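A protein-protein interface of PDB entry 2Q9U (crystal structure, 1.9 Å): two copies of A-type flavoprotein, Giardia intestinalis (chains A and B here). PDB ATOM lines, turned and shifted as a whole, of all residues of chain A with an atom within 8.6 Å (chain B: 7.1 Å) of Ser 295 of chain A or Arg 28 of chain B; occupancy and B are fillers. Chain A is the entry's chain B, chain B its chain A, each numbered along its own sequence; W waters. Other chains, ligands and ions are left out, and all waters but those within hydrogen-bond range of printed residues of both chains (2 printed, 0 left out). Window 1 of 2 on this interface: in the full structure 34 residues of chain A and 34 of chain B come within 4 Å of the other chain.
The backbone carbonyl oxygen (O) of Ser 295 of chain A lies within hydrogen-bond range of the guanidinium group (NH2) of Arg 28 of chain B, 3.0 Å away. OE1 of Glu 292 of chain A lies close to SD of Met 26 of chain B (3.4 Å). The side-chain sulfur (SD) of Met 26 of chain B sits close to a ring nitrogen (ND1) of His 271 of chain A (3.7 Å).
The backbone carbonyl oxygen of Trp 25 of chain B sits at hydrogen-bond distance from the guanidinium group of Arg 28 of chain B. N of Thr 35 of chain B is in hydrogen-bond range of O of Arg 28 of chain B, at 2.8 Å. A ring nitrogen (ND1) of His 271 of chain A lies within hydrogen-bond range of the side-chain carboxylate (OE1) of Glu 292 of chain A (2.7 Å). OG of Ser 295 of chain A is in hydrogen-bond range of O of Glu 292 of chain A, at 3.2 Å.
Val 289 of chain A touches Trp 25 of chain B. Leu 290 of chain A touches Trp 25 of chain B. Ser 295 of chain A touches Met 26 of chain B (CB to O, 3.4 Å).
Ser 295 of chain A touches two residues of chain B. Of chain A, only Ser 295 (3.0 Å) comes within 4 Å of Arg 28 of chain B. No residue of chain A comes within 4 Å of Val 27 of chain B. Of the printed residues of chain B, Val 289 of chain A touches Trp 25. Of the printed residues of chain A, Trp 25 of chain B touches Val 289 and Leu 290. His 34 of chain B touches none of the printed residues of chain A. The nearest residue of chain B that does not touch Ser 295 of chain A is Trp 25 of chain B (4.5 Å). The nearest printed residue of chain B that does not touch His 271 of chain A is Trp 25 of chain B (5.2 Å).
Of the 17 printed residues of chain A, 5 touch a printed residue of chain B. Among the printed residues, no Asp or Glu carboxylate lies within 4 Å of a Lys or Arg side-chain nitrogen of the other chain.
Position printed for both chains: 36.
Water W2 lies within hydrogen-bond range of O of Leu 290 of chain A (2.9 Å) and NH2 of Arg 28 of chain B (3.3 Å). Water W1 bridges the backbone carbonyl oxygen of Ser 295 of chain A (3.0 Å) and the guanidinium group of Arg 28 of chain B (3.4 Å).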
ATOM      1  N   ASP A  36      11.217   5.692 -28.002  1.00  0.00           N
ATOM      2  CA  ASP A  36      10.384   6.684 -28.697  1.00  0.00           C
ATOM      3  C   ASP A  36      11.237   7.715 -29.400  1.00  0.00           C
ATOM      4  O   ASP A  36      10.788   8.341 -30.376  1.00  0.00           O
ATOM      5  CB  ASP A  36       9.445   7.434 -27.738  1.00  0.00           C
ATOM      6  CG  ASP A  36       8.324   6.555 -27.162  1.00  0.00           C
ATOM      7  OD1 ASP A  36       8.148   5.411 -27.588  1.00  0.00           O
ATOM      8  OD2 ASP A  36       7.630   7.052 -26.250  1.00  0.00           O
ATOM      9  N   LEU A 263      -2.403   1.187 -13.973  1.00  0.00           N
ATOM     10  CA  LEU A 263      -3.664   0.472 -13.975  1.00  0.00           C
ATOM     11  C   LEU A 263      -4.100   0.144 -15.373  1.00  0.00           C
ATOM     12  O   LEU A 263      -3.508   0.622 -16.341  1.00  0.00           O
ATOM     13  CB  LEU A 263      -4.760   1.302 -13.281  1.00  0.00           C
ATOM     14  CG  LEU A 263      -5.413   2.472 -14.059  1.00  0.00           C
ATOM     15  CD1 LEU A 263      -6.807   2.706 -13.512  1.00  0.00           C
ATOM     16  CD2 LEU A 263      -4.574   3.703 -13.917  1.00  0.00           C
ATOM     17  N   ASP A 264      -5.123  -0.697 -15.463  1.00  0.00           N
ATOM     18  CA  ASP A 264      -5.910  -0.779 -16.694  1.00  0.00           C
ATOM     19  C   ASP A 264      -7.372  -0.782 -16.246  1.00  0.00           C
ATOM     20  O   ASP A 264      -7.672  -0.904 -15.035  1.00  0.00           O
ATOM     21  CB  ASP A 264      -5.549  -2.012 -17.531  1.00  0.00           C
ATOM     22  CG  ASP A 264      -5.801  -1.797 -19.041  1.00  0.00           C
ATOM     23  OD1 ASP A 264      -6.538  -0.840 -19.393  1.00  0.00           O
ATOM     24  OD2 ASP A 264      -5.257  -2.581 -19.872  1.00  0.00           O
ATOM     25  N   HIS A 271     -10.569   3.454 -13.255  1.00  0.00           N
ATOM     26  CA  HIS A 271      -9.959   4.739 -13.646  1.00  0.00           C
ATOM     27  C   HIS A 271     -10.466   5.949 -12.817  1.00  0.00           C
ATOM     28  O   HIS A 271      -9.663   6.747 -12.322  1.00  0.00           O
ATOM     29  CB  HIS A 271     -10.123   4.995 -15.146  1.00  0.00           C
ATOM     30  CG  HIS A 271      -9.537   6.301 -15.591  1.00  0.00           C
ATOM     31  ND1 HIS A 271      -8.221   6.432 -15.979  1.00  0.00           N
ATOM     32  CD2 HIS A 271     -10.072   7.546 -15.651  1.00  0.00           C
ATOM     33  CE1 HIS A 271      -7.982   7.694 -16.299  1.00  0.00           C
ATOM     34  NE2 HIS A 271      -9.086   8.389 -16.111  1.00  0.00           N
ATOM     35  N   VAL A 289       1.508  10.756 -10.946  1.00  0.00           N
ATOM     36  CA  VAL A 289       1.506  10.339 -12.345  1.00  0.00           C
ATOM     37  C   VAL A 289       0.502   9.181 -12.472  1.00  0.00           C
ATOM     38  O   VAL A 289       0.503   8.225 -11.683  1.00  0.00           O
ATOM     39  CB  VAL A 289       2.917   9.905 -12.801  1.00  0.00           C
ATOM     40  CG1 VAL A 289       2.901   9.205 -14.191  1.00  0.00           C
ATOM     41  CG2 VAL A 289       3.902  11.129 -12.795  1.00  0.00           C
ATOM     42  N   LEU A 290      -0.348   9.269 -13.469  1.00  0.00           N
ATOM     43  CA  LEU A 290      -1.231   8.142 -13.750  1.00  0.00           C
ATOM     44  C   LEU A 290      -0.889   7.499 -15.082  1.00  0.00           C
ATOM     45  O   LEU A 290      -0.840   8.192 -16.141  1.00  0.00           O
ATOM     46  CB  LEU A 290      -2.694   8.594 -13.712  1.00  0.00           C
ATOM     47  CG  LEU A 290      -3.744   7.502 -14.005  1.00  0.00           C
ATOM     48  CD1 LEU A 290      -4.959   7.712 -13.145  1.00  0.00           C
ATOM     49  CD2 LEU A 290      -4.139   7.418 -15.477  1.00  0.00           C
ATOM     50  N   LEU A 291      -0.704   6.176 -15.050  1.00  0.00           N
ATOM     51  CA  LEU A 291      -0.305   5.431 -16.218  1.00  0.00           C
ATOM     52  C   LEU A 291      -1.328   4.357 -16.494  1.00  0.00           C
ATOM     53  O   LEU A 291      -1.447   3.426 -15.712  1.00  0.00           O
ATOM     54  CB  LEU A 291       1.074   4.784 -16.008  1.00  0.00           C
ATOM     55  CG  LEU A 291       2.267   5.714 -15.708  1.00  0.00           C
ATOM     56  CD1 LEU A 291       3.536   4.891 -15.526  1.00  0.00           C
ATOM     57  CD2 LEU A 291       2.457   6.762 -16.840  1.00  0.00           C
ATOM     58  N   GLU A 292      -2.045   4.487 -17.610  1.00  0.00           N
ATOM     59  CA  GLU A 292      -3.054   3.503 -17.976  1.00  0.00           C
ATOM     60  C   GLU A 292      -2.530   2.708 -19.133  1.00  0.00           C
ATOM     61  O   GLU A 292      -2.132   3.279 -20.168  1.00  0.00           O
ATOM     62  CB  GLU A 292      -4.396   4.158 -18.328  1.00  0.00           C
ATOM     63  CG  GLU A 292      -5.526   3.134 -18.425  1.00  0.00           C
ATOM     64  CD  GLU A 292      -6.827   3.593 -17.754  1.00  0.00           C
ATOM     65  OE1 GLU A 292      -6.781   4.328 -16.735  1.00  0.00           O
ATOM     66  OE2 GLU A 292      -7.901   3.215 -18.258  1.00  0.00           O
ATOM     67  N   MET A 293      -2.530   1.385 -18.981  1.00  0.00           N
ATOM     68  CA  MET A 293      -1.791   0.536 -19.913  1.00  0.00           C
ATOM     69  C   MET A 293      -2.249   0.633 -21.372  1.00  0.00           C
ATOM     70  O   MET A 293      -1.433   0.473 -22.267  1.00  0.00           O
ATOM     71  CB  MET A 293      -1.739  -0.915 -19.446  1.00  0.00           C
ATOM     72  CG  MET A 293      -1.006  -1.123 -18.123  1.00  0.00           C
ATOM     73  SD  MET A 293       0.608  -0.307 -18.000  1.00  0.00           S
ATOM     74  CE  MET A 293       1.589  -0.982 -19.315  1.00  0.00           C
ATOM     75  N   THR A 294      -3.537   0.907 -21.590  1.00  0.00           N
ATOM     76  CA  THR A 294      -4.079   1.207 -22.936  1.00  0.00           C
ATOM     77  C   THR A 294      -3.466   2.459 -23.605  1.00  0.00           C
ATOM     78  O   THR A 294      -3.570   2.636 -24.828  1.00  0.00           O
ATOM     79  CB  THR A 294      -5.632   1.341 -22.932  1.00  0.00           C
ATOM     80  OG1 THR A 294      -6.061   2.290 -21.955  1.00  0.00           O
ATOM     81  CG2 THR A 294      -6.274   0.027 -22.582  1.00  0.00           C
ATOM     82  N   SER A 295      -2.831   3.328 -22.817  1.00  0.00           N
ATOM     83  CA  SER A 295      -2.182   4.515 -23.372  1.00  0.00           C
ATOM     84  C   SER A 295      -0.744   4.663 -22.879  1.00  0.00           C
ATOM     85  O   SER A 295      -0.105   5.695 -23.076  1.00  0.00           O
ATOM     86  CB  SER A 295      -2.989   5.780 -23.066  1.00  0.00           C
ATOM     87  OG  SER A 295      -3.209   5.908 -21.695  1.00  0.00           O
ATOM     88  N   SER A 296      -0.218   3.623 -22.254  1.00  0.00           N
ATOM     89  CA  SER A 296       1.157   3.690 -21.773  1.00  0.00           C
ATOM     90  C   SER A 296       1.932   2.455 -22.231  1.00  0.00           C
ATOM     91  O   SER A 296       1.492   1.708 -23.135  1.00  0.00           O
ATOM     92  CB  SER A 296       1.185   3.864 -20.238  1.00  0.00           C
ATOM     93  OG  SER A 296       2.499   4.178 -19.793  1.00  0.00           O
ATOM     94  N   ASP A 297       3.104   2.242 -21.658  1.00  0.00           N
ATOM     95  CA  ASP A 297       3.835   1.028 -21.972  1.00  0.00           C
ATOM     96  C   ASP A 297       4.753   0.671 -20.831  1.00  0.00           C
ATOM     97  O   ASP A 297       4.952   1.484 -19.894  1.00  0.00           O
ATOM     98  CB  ASP A 297       4.611   1.162 -23.305  1.00  0.00           C
ATOM     99  CG  ASP A 297       5.560   2.352 -23.306  1.00  0.00           C
ATOM    100  OD1 ASP A 297       6.496   2.336 -22.492  1.00  0.00           O
ATOM    101  OD2 ASP A 297       5.367   3.310 -24.111  1.00  0.00           O
ATOM    102  N   ILE A 298       5.306  -0.534 -20.875  1.00  0.00           N
ATOM    103  CA  ILE A 298       6.094  -1.002 -19.716  1.00  0.00           C
ATOM    104  C   ILE A 298       7.345  -0.177 -19.476  1.00  0.00           C
ATOM    105  O   ILE A 298       7.804  -0.067 -18.357  1.00  0.00           O
ATOM    106  CB  ILE A 298       6.460  -2.490 -19.809  1.00  0.00           C
ATOM    107  CG1 ILE A 298       7.169  -2.807 -21.158  1.00  0.00           C
ATOM    108  CG2 ILE A 298       5.206  -3.355 -19.496  1.00  0.00           C
ATOM    109  CD1 ILE A 298       7.780  -4.239 -21.212  1.00  0.00           C
ATOM    110  N   LYS A 300       7.624   3.117 -19.825  1.00  0.00           N
ATOM    111  CA  LYS A 300       7.198   4.258 -18.999  1.00  0.00           C
ATOM    112  C   LYS A 300       6.849   3.851 -17.565  1.00  0.00           C
ATOM    113  O   LYS A 300       7.098   4.610 -16.605  1.00  0.00           O
ATOM    114  CB  LYS A 300       6.050   5.011 -19.686  1.00  0.00           C
ATOM    115  CG  LYS A 300       6.579   5.554 -21.031  1.00  0.00           C
ATOM    116  CD  LYS A 300       5.620   6.243 -21.918  1.00  0.00           C
ATOM    117  CE  LYS A 300       6.457   6.772 -23.148  1.00  0.00           C
ATOM    118  NZ  LYS A 300       7.057   5.619 -23.961  1.00  0.00           N
ATOM    119  N   VAL A 301       6.289   2.655 -17.404  1.00  0.00           N
ATOM    120  CA  VAL A 301       6.013   2.144 -16.027  1.00  0.00           C
ATOM    121  C   VAL A 301       7.339   2.033 -15.243  1.00  0.00           C
ATOM    122  O   VAL A 301       7.426   2.441 -14.068  1.00  0.00           O
ATOM    123  CB  VAL A 301       5.267   0.774 -16.079  1.00  0.00           C
ATOM    124  CG1 VAL A 301       5.135   0.110 -14.651  1.00  0.00           C
ATOM    125  CG2 VAL A 301       3.873   0.951 -16.713  1.00  0.00           C
ATOM    126  N   SER A 325      -2.461  -6.768 -19.122  1.00  0.00           N
ATOM    127  CA  SER A 325      -1.531  -5.644 -19.222  1.00  0.00           C
ATOM    128  C   SER A 325      -0.910  -5.311 -17.829  1.00  0.00           C
ATOM    129  O   SER A 325       0.258  -4.910 -17.722  1.00  0.00           O
ATOM    130  CB  SER A 325      -2.243  -4.417 -19.777  1.00  0.00           C
ATOM    131  OG  SER A 325      -3.253  -4.017 -18.850  1.00  0.00           O
ATOM    132  N   ASP B  24      -6.048  15.247 -18.738  1.00  0.00           N
ATOM    133  CA  ASP B  24      -6.418  14.162 -19.653  1.00  0.00           C
ATOM    134  C   ASP B  24      -5.167  13.270 -19.812  1.00  0.00           C
ATOM    135  O   ASP B  24      -4.367  13.406 -20.754  1.00  0.00           O
ATOM    136  CB  ASP B  24      -6.926  14.721 -20.996  1.00  0.00           C
ATOM    137  CG  ASP B  24      -7.624  13.670 -21.857  1.00  0.00           C
ATOM    138  OD1 ASP B  24      -7.446  12.464 -21.600  1.00  0.00           O
ATOM    139  OD2 ASP B  24      -8.300  14.050 -22.852  1.00  0.00           O
ATOM    140  N   TRP B  25      -5.001  12.373 -18.853  1.00  0.00           N
ATOM    141  CA  TRP B  25      -3.845  11.466 -18.803  1.00  0.00           C
ATOM    142  C   TRP B  25      -3.761  10.551 -20.039  1.00  0.00           C
ATOM    143  O   TRP B  25      -2.673  10.257 -20.533  1.00  0.00           O
ATOM    144  CB  TRP B  25      -3.919  10.616 -17.527  1.00  0.00           C
ATOM    145  CG  TRP B  25      -3.728  11.439 -16.252  1.00  0.00           C
ATOM    146  CD1 TRP B  25      -4.703  11.859 -15.370  1.00  0.00           C
ATOM    147  CD2 TRP B  25      -2.489  11.951 -15.752  1.00  0.00           C
ATOM    148  NE1 TRP B  25      -4.133  12.590 -14.349  1.00  0.00           N
ATOM    149  CE2 TRP B  25      -2.774  12.640 -14.549  1.00  0.00           C
ATOM    150  CE3 TRP B  25      -1.151  11.878 -16.197  1.00  0.00           C
ATOM    151  CZ2 TRP B  25      -1.781  13.245 -13.787  1.00  0.00           C
ATOM    152  CZ3 TRP B  25      -0.162  12.483 -15.425  1.00  0.00           C
ATOM    153  CH2 TRP B  25      -0.483  13.162 -14.248  1.00  0.00           C
ATOM    154  N   MET B  26      -4.895  10.146 -20.569  1.00  0.00           N
ATOM    155  CA  MET B  26      -4.921   9.071 -21.562  1.00  0.00           C
ATOM    156  C   MET B  26      -4.943   9.462 -23.030  1.00  0.00           C
ATOM    157  O   MET B  26      -4.673   8.608 -23.903  1.00  0.00           O
ATOM    158  CB  MET B  26      -6.097   8.158 -21.260  1.00  0.00           C
ATOM    159  CG  MET B  26      -5.930   7.550 -19.882  1.00  0.00           C
ATOM    160  SD  MET B  26      -7.158   6.331 -19.501  1.00  0.00           S
ATOM    161  CE  MET B  26      -8.607   7.298 -19.446  1.00  0.00           C
ATOM    162  N   VAL B  27      -5.274  10.725 -23.318  1.00  0.00           N
ATOM    163  CA  VAL B  27      -5.450  11.131 -24.714  1.00  0.00           C
ATOM    164  C   VAL B  27      -4.128  10.981 -25.473  1.00  0.00           C
ATOM    165  O   VAL B  27      -3.059  11.409 -24.991  1.00  0.00           O
ATOM    166  CB  VAL B  27      -6.090  12.536 -24.899  1.00  0.00           C
ATOM    167  CG1 VAL B  27      -5.210  13.675 -24.361  1.00  0.00           C
ATOM    168  CG2 VAL B  27      -6.463  12.780 -26.384  1.00  0.00           C
ATOM    169  N   ARG B  28      -4.199  10.337 -26.633  1.00  0.00           N
ATOM    170  CA  ARG B  28      -2.996  10.148 -27.471  1.00  0.00           C
ATOM    171  C   ARG B  28      -3.128  10.711 -28.877  1.00  0.00           C
ATOM    172  O   ARG B  28      -2.122  11.018 -29.521  1.00  0.00           O
ATOM    173  CB  ARG B  28      -2.553   8.668 -27.520  1.00  0.00           C
ATOM    174  CG  ARG B  28      -1.989   8.153 -26.186  1.00  0.00           C
ATOM    175  CD  ARG B  28      -0.648   8.793 -25.804  1.00  0.00           C
ATOM    176  NE  ARG B  28      -0.253   8.370 -24.456  1.00  0.00           N
ATOM    177  CZ  ARG B  28      -0.579   9.001 -23.323  1.00  0.00           C
ATOM    178  NH1 ARG B  28      -1.254  10.150 -23.354  1.00  0.00           N
ATOM    179  NH2 ARG B  28      -0.199   8.499 -22.147  1.00  0.00           N
ATOM    180  N   ILE B  29      -4.362  10.833 -29.347  1.00  0.00           N
ATOM    181  CA  ILE B  29      -4.637  11.470 -30.634  1.00  0.00           C
ATOM    182  C   ILE B  29      -5.735  12.489 -30.381  1.00  0.00           C
ATOM    183  O   ILE B  29      -6.797  12.154 -29.845  1.00  0.00           O
ATOM    184  CB  ILE B  29      -5.066  10.459 -31.748  1.00  0.00           C
ATOM    185  CG1 ILE B  29      -4.018   9.363 -31.952  1.00  0.00           C
ATOM    186  CG2 ILE B  29      -5.333  11.214 -33.099  1.00  0.00           C
ATOM    187  CD1 ILE B  29      -2.718   9.841 -32.533  1.00  0.00           C
ATOM    188  N   PHE B  30      -5.467  13.740 -30.731  1.00  0.00           N
ATOM    189  CA  PHE B  30      -6.400  14.813 -30.430  1.00  0.00           C
ATOM    190  C   PHE B  30      -6.535  15.679 -31.664  1.00  0.00           C
ATOM    191  O   PHE B  30      -5.639  16.467 -31.988  1.00  0.00           O
ATOM    192  CB  PHE B  30      -5.907  15.627 -29.221  1.00  0.00           C
ATOM    193  CG  PHE B  30      -6.767  16.826 -28.896  1.00  0.00           C
ATOM    194  CD1 PHE B  30      -8.163  16.730 -28.910  1.00  0.00           C
ATOM    195  CD2 PHE B  30      -6.184  18.047 -28.628  1.00  0.00           C
ATOM    196  CE1 PHE B  30      -8.976  17.852 -28.631  1.00  0.00           C
ATOM    197  CE2 PHE B  30      -6.966  19.175 -28.324  1.00  0.00           C
ATOM    198  CZ  PHE B  30      -8.360  19.079 -28.328  1.00  0.00           C
ATOM    199  N   GLY B  32      -6.180  14.659 -34.567  1.00  0.00           N
ATOM    200  CA  GLY B  32      -5.008  14.313 -35.364  1.00  0.00           C
ATOM    201  C   GLY B  32      -3.656  14.740 -34.811  1.00  0.00           C
ATOM    202  O   GLY B  32      -2.622  14.408 -35.399  1.00  0.00           O
ATOM    203  N   TYR B  33      -3.638  15.471 -33.693  1.00  0.00           N
ATOM    204  CA  TYR B  33      -2.368  15.814 -33.005  1.00  0.00           C
ATOM    205  C   TYR B  33      -1.913  14.608 -32.168  1.00  0.00           C
ATOM    206  O   TYR B  33      -2.679  14.064 -31.363  1.00  0.00           O
ATOM    207  CB  TYR B  33      -2.563  17.054 -32.112  1.00  0.00           C
ATOM    208  CG  TYR B  33      -1.337  17.653 -31.407  1.00  0.00           C
ATOM    209  CD1 TYR B  33      -0.648  16.957 -30.406  1.00  0.00           C
ATOM    210  CD2 TYR B  33      -0.922  18.944 -31.695  1.00  0.00           C
ATOM    211  CE1 TYR B  33       0.460  17.520 -29.746  1.00  0.00           C
ATOM    212  CE2 TYR B  33       0.171  19.520 -31.045  1.00  0.00           C
ATOM    213  CZ  TYR B  33       0.852  18.808 -30.083  1.00  0.00           C
ATOM    214  OH  TYR B  33       1.896  19.390 -29.448  1.00  0.00           O
ATOM    215  N   HIS B  34      -0.675  14.178 -32.351  1.00  0.00           N
ATOM    216  CA  HIS B  34      -0.187  13.057 -31.553  1.00  0.00           C
ATOM    217  C   HIS B  34       0.206  13.585 -30.188  1.00  0.00           C
ATOM    218  O   HIS B  34       1.305  14.127 -30.030  1.00  0.00           O
ATOM    219  CB  HIS B  34       0.991  12.381 -32.239  1.00  0.00           C
ATOM    220  CG  HIS B  34       0.578  11.428 -33.308  1.00  0.00           C
ATOM    221  ND1 HIS B  34      -0.101  11.829 -34.436  1.00  0.00           N
ATOM    222  CD2 HIS B  34       0.753  10.091 -33.424  1.00  0.00           C
ATOM    223  CE1 HIS B  34      -0.334  10.776 -35.204  1.00  0.00           C
ATOM    224  NE2 HIS B  34       0.168   9.708 -34.607  1.00  0.00           N
ATOM    225  N   THR B  35      -0.704  13.463 -29.217  1.00  0.00           N
ATOM    226  CA  THR B  35      -0.469  14.034 -27.896  1.00  0.00           C
ATOM    227  C   THR B  35       0.250  12.970 -27.068  1.00  0.00           C
ATOM    228  O   THR B  35      -0.370  12.323 -26.246  1.00  0.00           O
ATOM    229  CB  THR B  35      -1.794  14.493 -27.180  1.00  0.00           C
ATOM    230  OG1 THR B  35      -2.745  13.425 -27.176  1.00  0.00           O
ATOM    231  CG2 THR B  35      -2.408  15.683 -27.893  1.00  0.00           C
ATOM    232  N   ASP B  36       1.553  12.789 -27.305  1.00  0.00           N
ATOM    233  CA  ASP B  36       2.297  11.674 -26.690  1.00  0.00           C
ATOM    234  C   ASP B  36       2.320  11.782 -25.172  1.00  0.00           C
ATOM    235  O   ASP B  36       2.436  10.765 -24.474  1.00  0.00           O
ATOM    236  CB  ASP B  36       3.744  11.639 -27.185  1.00  0.00           C
ATOM    237  CG  ASP B  36       3.858  11.221 -28.644  1.00  0.00           C
ATOM    238  OD1 ASP B  36       2.843  10.850 -29.266  1.00  0.00           O
ATOM    239  OD2 ASP B  36       4.986  11.260 -29.167  1.00  0.00           O
ATOM    240  N   GLU B  37       2.216  13.018 -24.686  1.00  0.00           N
ATOM    241  CA  GLU B  37       2.182  13.286 -23.244  1.00  0.00           C
ATOM    242  C   GLU B  37       0.824  13.702 -22.661  1.00  0.00           C
ATOM    243  O   GLU B  37       0.793  14.281 -21.585  1.00  0.00           O
ATOM    244  CB  GLU B  37       3.286  14.275 -22.869  1.00  0.00           C
ATOM    245  CG  GLU B  37       4.648  13.738 -23.331  1.00  0.00           C
ATOM    246  CD  GLU B  37       5.796  14.529 -22.793  1.00  0.00           C
ATOM    247  OE1 GLU B  37       5.857  14.762 -21.568  1.00  0.00           O
ATOM    248  OE2 GLU B  37       6.633  14.914 -23.622  1.00  0.00           O
ATOM    249  N   GLY B  38      -0.268  13.345 -23.337  1.00  0.00           N
ATOM    250  CA  GLY B  38      -1.621  13.667 -22.858  1.00  0.00           C
ATOM    251  C   GLY B  38      -1.868  15.167 -23.013  1.00  0.00           C
ATOM    252  O   GLY B  38      -1.187  15.832 -23.797  1.00  0.00           O
ATOM    253  N   SER B  39      -2.847  15.703 -22.279  1.00  0.00           N
ATOM    254  CA  SER B  39      -3.077  17.150 -22.267  1.00  0.00           C
ATOM    255  C   SER B  39      -3.821  17.452 -20.975  1.00  0.00           C
ATOM    256  O   SER B  39      -3.967  16.586 -20.121  1.00  0.00           O
ATOM    257  CB  SER B  39      -3.933  17.540 -23.480  1.00  0.00           C
ATOM    258  OG  SER B  39      -4.063  18.959 -23.621  1.00  0.00           O
ATOM    259  N   ALA B 178       0.099  16.506 -19.870  1.00  0.00           N
ATOM    260  CA  ALA B 178      -0.590  16.040 -18.672  1.00  0.00           C
ATOM    261  C   ALA B 178       0.417  15.921 -17.522  1.00  0.00           C
ATOM    262  O   ALA B 178       1.379  15.160 -17.629  1.00  0.00           O
ATOM    263  CB  ALA B 178      -1.299  14.644 -18.901  1.00  0.00           C
HETATM  264  O   HOH W   1       2.657   6.942 -23.230  1.00  0.00           O
HETATM  265  O   HOH W   2       0.015   8.502 -18.888  1.00  0.00           O
